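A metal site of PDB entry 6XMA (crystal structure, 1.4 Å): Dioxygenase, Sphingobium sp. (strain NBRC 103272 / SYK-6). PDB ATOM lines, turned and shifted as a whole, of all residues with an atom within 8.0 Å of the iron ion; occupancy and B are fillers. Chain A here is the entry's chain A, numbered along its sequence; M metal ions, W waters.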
ATOM      1  N   PHE A  59     -10.084  15.152 -11.877  1.00  0.00           N
ATOM      2  CA  PHE A  59      -9.457  13.913 -12.282  1.00  0.00           C
ATOM      3  C   PHE A  59     -10.303  13.137 -13.291  1.00  0.00           C
ATOM      4  O   PHE A  59      -9.864  12.064 -13.711  1.00  0.00           O
ATOM      5  CB  PHE A  59      -9.201  13.006 -11.062  1.00  0.00           C
ATOM      6  CG  PHE A  59      -8.013  13.397 -10.210  1.00  0.00           C
ATOM      7  CD1 PHE A  59      -7.272  14.545 -10.442  1.00  0.00           C
ATOM      8  CD2 PHE A  59      -7.652  12.575  -9.152  1.00  0.00           C
ATOM      9  CE1 PHE A  59      -6.187  14.862  -9.636  1.00  0.00           C
ATOM     10  CE2 PHE A  59      -6.567  12.886  -8.352  1.00  0.00           C
ATOM     11  CZ  PHE A  59      -5.848  14.032  -8.584  1.00  0.00           C
ATOM     12  N   THR A 121      -3.943  10.549 -17.288  1.00  0.00           N
ATOM     13  CA  THR A 121      -3.025  10.669 -16.145  1.00  0.00           C
ATOM     14  C   THR A 121      -1.559  10.692 -16.541  1.00  0.00           C
ATOM     15  O   THR A 121      -0.755  11.344 -15.860  1.00  0.00           O
ATOM     16  CB  THR A 121      -3.284   9.520 -15.156  1.00  0.00           C
ATOM     17  OG1 THR A 121      -4.643   9.591 -14.707  1.00  0.00           O
ATOM     18  CG2 THR A 121      -2.405   9.601 -13.920  1.00  0.00           C
ATOM     19  N   ASN A 122      -1.162  10.011 -17.607  1.00  0.00           N
ATOM     20  CA  ASN A 122       0.208  10.077 -18.076  1.00  0.00           C
ATOM     21  C   ASN A 122       0.245   9.991 -19.592  1.00  0.00           C
ATOM     22  O   ASN A 122      -0.643   9.408 -20.217  1.00  0.00           O
ATOM     23  CB  ASN A 122       1.052   8.968 -17.444  1.00  0.00           C
ATOM     24  CG  ASN A 122       2.525   9.309 -17.326  1.00  0.00           C
ATOM     25  OD1 ASN A 122       3.083  10.181 -18.022  1.00  0.00           O
ATOM     26  ND2 ASN A 122       3.188   8.574 -16.437  1.00  0.00           N
ATOM     27  N   GLU A 135      -5.445   4.448 -14.637  1.00  0.00           N
ATOM     28  CA  GLU A 135      -5.191   3.254 -13.848  1.00  0.00           C
ATOM     29  C   GLU A 135      -6.395   2.350 -13.648  1.00  0.00           C
ATOM     30  O   GLU A 135      -6.243   1.341 -12.959  1.00  0.00           O
ATOM     31  CB  GLU A 135      -4.638   3.673 -12.478  1.00  0.00           C
ATOM     32  CG  GLU A 135      -5.617   4.425 -11.602  1.00  0.00           C
ATOM     33  CD  GLU A 135      -4.928   5.284 -10.568  1.00  0.00           C
ATOM     34  OE1 GLU A 135      -4.055   6.099 -10.932  1.00  0.00           O
ATOM     35  OE2 GLU A 135      -5.312   5.172  -9.404  1.00  0.00           O
ATOM     36  N   ALA A 166      -0.879   4.120 -14.350  1.00  0.00           N
ATOM     37  CA  ALA A 166      -0.436   5.321 -15.049  1.00  0.00           C
ATOM     38  C   ALA A 166       0.931   5.798 -14.566  1.00  0.00           C
ATOM     39  O   ALA A 166       1.367   6.873 -14.962  1.00  0.00           O
ATOM     40  CB  ALA A 166      -1.492   6.417 -14.924  1.00  0.00           C
ATOM     41  N   HIS A 167       1.629   4.986 -13.754  1.00  0.00           N
ATOM     42  CA  HIS A 167       2.974   5.331 -13.283  1.00  0.00           C
ATOM     43  C   HIS A 167       3.981   4.246 -13.629  1.00  0.00           C
ATOM     44  O   HIS A 167       4.732   3.782 -12.747  1.00  0.00           O
ATOM     45  CB  HIS A 167       2.914   5.598 -11.777  1.00  0.00           C
ATOM     46  CG  HIS A 167       2.567   7.020 -11.453  1.00  0.00           C
ATOM     47  ND1 HIS A 167       3.463   8.045 -11.629  1.00  0.00           N
ATOM     48  CD2 HIS A 167       1.412   7.597 -11.040  1.00  0.00           C
ATOM     49  CE1 HIS A 167       2.886   9.188 -11.296  1.00  0.00           C
ATOM     50  NE2 HIS A 167       1.637   8.952 -10.950  1.00  0.00           N
ATOM     51  N   MET A 216      -6.460   3.251  -3.266  1.00  0.00           N
ATOM     52  CA  MET A 216      -5.833   3.836  -4.446  1.00  0.00           C
ATOM     53  C   MET A 216      -4.351   3.495  -4.476  1.00  0.00           C
ATOM     54  O   MET A 216      -3.555   4.096  -3.746  1.00  0.00           O
ATOM     55  CB  MET A 216      -6.005   5.355  -4.433  1.00  0.00           C
ATOM     56  CG  MET A 216      -5.666   5.921  -5.787  1.00  0.00           C
ATOM     57  SD  MET A 216      -5.379   7.714  -5.826  1.00  0.00           S
ATOM     58  CE  MET A 216      -6.968   8.361  -5.345  1.00  0.00           C
ATOM     59  N   HIS A 218      -1.897   4.202  -6.691  1.00  0.00           N
ATOM     60  CA  HIS A 218      -1.634   5.109  -7.808  1.00  0.00           C
ATOM     61  C   HIS A 218      -0.197   4.998  -8.299  1.00  0.00           C
ATOM     62  O   HIS A 218       0.053   5.081  -9.510  1.00  0.00           O
ATOM     63  CB  HIS A 218      -1.962   6.538  -7.324  1.00  0.00           C
ATOM     64  CG  HIS A 218      -1.680   7.608  -8.319  1.00  0.00           C
ATOM     65  ND1 HIS A 218      -2.412   7.755  -9.478  1.00  0.00           N
ATOM     66  CD2 HIS A 218      -0.772   8.604  -8.314  1.00  0.00           C
ATOM     67  CE1 HIS A 218      -1.936   8.779 -10.157  1.00  0.00           C
ATOM     68  NE2 HIS A 218      -0.945   9.325  -9.477  1.00  0.00           N
ATOM     69  N   ASP A 219       0.756   4.838  -7.384  1.00  0.00           N
ATOM     70  CA  ASP A 219       2.175   4.862  -7.727  1.00  0.00           C
ATOM     71  C   ASP A 219       2.857   3.775  -6.900  1.00  0.00           C
ATOM     72  O   ASP A 219       2.218   3.086  -6.092  1.00  0.00           O
ATOM     73  CB  ASP A 219       2.746   6.273  -7.483  1.00  0.00           C
ATOM     74  CG  ASP A 219       4.013   6.567  -8.260  1.00  0.00           C
ATOM     75  OD1 ASP A 219       4.574   5.667  -8.927  1.00  0.00           O
ATOM     76  OD2 ASP A 219       4.452   7.751  -8.177  1.00  0.00           O
ATOM     77  N   SER A 283       1.387   9.580  -1.911  1.00  0.00           N
ATOM     78  CA  SER A 283       0.892   9.187  -3.234  1.00  0.00           C
ATOM     79  C   SER A 283       2.050   8.838  -4.159  1.00  0.00           C
ATOM     80  O   SER A 283       2.119   7.701  -4.630  1.00  0.00           O
ATOM     81  CB  SER A 283       0.061  10.319  -3.818  1.00  0.00           C
ATOM     82  OG  SER A 283      -0.437   9.984  -5.113  1.00  0.00           O
ATOM     83  N   HIS A 284       2.931   9.764  -4.449  1.00  0.00           N
ATOM     84  CA  HIS A 284       3.938   9.583  -5.473  1.00  0.00           C
ATOM     85  C   HIS A 284       5.271   9.100  -4.927  1.00  0.00           C
ATOM     86  O   HIS A 284       5.589   9.277  -3.749  1.00  0.00           O
ATOM     87  CB  HIS A 284       4.152  10.891  -6.242  1.00  0.00           C
ATOM     88  CG  HIS A 284       3.025  11.219  -7.146  1.00  0.00           C
ATOM     89  ND1 HIS A 284       2.328  12.409  -7.085  1.00  0.00           N
ATOM     90  CD2 HIS A 284       2.449  10.498  -8.141  1.00  0.00           C
ATOM     91  CE1 HIS A 284       1.382  12.406  -7.996  1.00  0.00           C
ATOM     92  NE2 HIS A 284       1.412  11.246  -8.640  1.00  0.00           N
ATOM     93  N   VAL A 285       6.030   8.462  -5.796  1.00  0.00           N
ATOM     94  CA  VAL A 285       7.370   7.963  -5.498  1.00  0.00           C
ATOM     95  C   VAL A 285       8.392   8.759  -6.298  1.00  0.00           C
ATOM     96  O   VAL A 285       8.344   8.794  -7.531  1.00  0.00           O
ATOM     97  CB  VAL A 285       7.463   6.459  -5.808  1.00  0.00           C
ATOM     98  CG1 VAL A 285       8.903   5.981  -5.680  1.00  0.00           C
ATOM     99  CG2 VAL A 285       6.574   5.685  -4.859  1.00  0.00           C
ATOM    100  N   PHE A 307      -6.369  14.766  -0.868  1.00  0.00           N
ATOM    101  CA  PHE A 307      -7.382  14.882  -1.911  1.00  0.00           C
ATOM    102  C   PHE A 307      -8.686  15.428  -1.320  1.00  0.00           C
ATOM    103  O   PHE A 307      -9.509  14.643  -0.816  1.00  0.00           O
ATOM    104  CB  PHE A 307      -7.667  13.541  -2.573  1.00  0.00           C
ATOM    105  CG  PHE A 307      -6.484  12.867  -3.197  1.00  0.00           C
ATOM    106  CD1 PHE A 307      -5.680  13.528  -4.111  1.00  0.00           C
ATOM    107  CD2 PHE A 307      -6.229  11.549  -2.915  1.00  0.00           C
ATOM    108  CE1 PHE A 307      -4.610  12.881  -4.696  1.00  0.00           C
ATOM    109  CE2 PHE A 307      -5.180  10.886  -3.513  1.00  0.00           C
ATOM    110  CZ  PHE A 307      -4.377  11.562  -4.413  1.00  0.00           C
ATOM    111  N   GLU A 353       5.395  18.273  -4.216  1.00  0.00           N
ATOM    112  CA  GLU A 353       4.819  17.073  -4.790  1.00  0.00           C
ATOM    113  C   GLU A 353       5.351  16.951  -6.223  1.00  0.00           C
ATOM    114  O   GLU A 353       6.300  17.654  -6.615  1.00  0.00           O
ATOM    115  CB  GLU A 353       3.289  17.141  -4.777  1.00  0.00           C
ATOM    116  CG  GLU A 353       2.651  16.122  -3.844  1.00  0.00           C
ATOM    117  CD  GLU A 353       2.617  14.710  -4.400  1.00  0.00           C
ATOM    118  OE1 GLU A 353       2.106  13.811  -3.705  1.00  0.00           O
ATOM    119  OE2 GLU A 353       3.048  14.494  -5.552  1.00  0.00           O
ATOM    120  N   PHE A 354       4.755  16.053  -6.993  1.00  0.00           N
ATOM    121  CA  PHE A 354       5.194  15.760  -8.348  1.00  0.00           C
ATOM    122  C   PHE A 354       6.723  15.512  -8.410  1.00  0.00           C
ATOM    123  O   PHE A 354       7.421  16.136  -9.223  1.00  0.00           O
ATOM    124  CB  PHE A 354       4.793  16.863  -9.305  1.00  0.00           C
ATOM    125  CG  PHE A 354       3.364  16.829  -9.717  1.00  0.00           C
ATOM    126  CD1 PHE A 354       2.905  15.905 -10.637  1.00  0.00           C
ATOM    127  CD2 PHE A 354       2.476  17.778  -9.208  1.00  0.00           C
ATOM    128  CE1 PHE A 354       1.583  15.933 -11.063  1.00  0.00           C
ATOM    129  CE2 PHE A 354       1.155  17.796  -9.611  1.00  0.00           C
ATOM    130  CZ  PHE A 354       0.703  16.879 -10.551  1.00  0.00           C
ATOM    131  N   PRO A 355       7.226  14.590  -7.625  1.00  0.00           N
ATOM    132  CA  PRO A 355       8.666  14.309  -7.603  1.00  0.00           C
ATOM    133  C   PRO A 355       9.133  13.616  -8.877  1.00  0.00           C
ATOM    134  O   PRO A 355       8.444  12.750  -9.416  1.00  0.00           O
ATOM    135  CB  PRO A 355       8.803  13.355  -6.425  1.00  0.00           C
ATOM    136  CG  PRO A 355       7.500  12.604  -6.404  1.00  0.00           C
ATOM    137  CD  PRO A 355       6.458  13.647  -6.799  1.00  0.00           C
ATOM    138  N   GLU A 418       4.154  19.722 -13.624  1.00  0.00           N
ATOM    139  CA  GLU A 418       5.189  18.750 -13.284  1.00  0.00           C
ATOM    140  C   GLU A 418       6.434  18.938 -14.154  1.00  0.00           C
ATOM    141  O   GLU A 418       6.322  18.983 -15.384  1.00  0.00           O
ATOM    142  CB  GLU A 418       4.656  17.334 -13.480  1.00  0.00           C
ATOM    143  CG  GLU A 418       5.702  16.251 -13.171  1.00  0.00           C
ATOM    144  CD  GLU A 418       5.277  14.882 -13.646  1.00  0.00           C
ATOM    145  OE1 GLU A 418       5.003  14.711 -14.855  1.00  0.00           O
ATOM    146  OE2 GLU A 418       5.212  13.963 -12.802  1.00  0.00           O
ATOM    147  N   LEU A 475      -1.392  16.421 -15.519  1.00  0.00           N
ATOM    148  CA  LEU A 475      -0.906  15.326 -14.692  1.00  0.00           C
ATOM    149  C   LEU A 475       0.519  15.032 -15.131  1.00  0.00           C
ATOM    150  O   LEU A 475       1.377  15.911 -15.029  1.00  0.00           O
ATOM    151  CB  LEU A 475      -1.906  14.183 -14.670  1.00  0.00           C
ATOM    152  CG  LEU A 475      -3.126  14.559 -13.801  1.00  0.00           C
ATOM    153  CD1 LEU A 475      -4.293  13.576 -14.009  1.00  0.00           C
ATOM    154  CD2 LEU A 475      -2.745  14.686 -12.308  1.00  0.00           C
ATOM    155  N   HIS A 476       0.831  13.833 -15.602  1.00  0.00           N
ATOM    156  CA  HIS A 476       2.227  13.444 -15.784  1.00  0.00           C
ATOM    157  C   HIS A 476       2.670  13.528 -17.239  1.00  0.00           C
ATOM    158  O   HIS A 476       1.858  13.478 -18.168  1.00  0.00           O
ATOM    159  CB  HIS A 476       2.463  12.053 -15.181  1.00  0.00           C
ATOM    160  CG  HIS A 476       2.097  12.001 -13.740  1.00  0.00           C
ATOM    161  ND1 HIS A 476       2.882  12.560 -12.761  1.00  0.00           N
ATOM    162  CD2 HIS A 476       0.958  11.604 -13.122  1.00  0.00           C
ATOM    163  CE1 HIS A 476       2.260  12.458 -11.587  1.00  0.00           C
ATOM    164  NE2 HIS A 476       1.120  11.832 -11.778  1.00  0.00           N
HETATM  165 FE    FE M   1       0.306  10.649 -10.305  1.00  0.00          FE
HETATM  166  O   HOH W   1      -1.145  12.323  -9.851  1.00  0.00           O
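A ring nitrogen (ND1) of His 218 sits at hydrogen-bond distance from the side-chain carboxylate of Glu 135 (2.7 Å).
The backbone NH (N) of His 476 sits at hydrogen-bond distance from the backbone carbonyl oxygen (O) of Thr 121, at 3.0 Å.
The side-chain carboxylate (OE2) of Glu 418 is in hydrogen-bond range of a ring nitrogen (ND1) of His 476 (2.7 Å).
The side-chain carboxylate (OE2) of Glu 353 sits at hydrogen-bond distance from a ring nitrogen (ND1) of His 284 (2.7 Å).
Within 4 Å of the iron ion: His 167, His 218, His 284 and His 476.
The iron ion is bound by NE2 of His 218 (2.0 Å), NE2 of His 476 (2.1 Å), NE2 of His 284 (2.1 Å), NE2 of His 167 (2.3 Å) and water W1 (2.3 Å).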
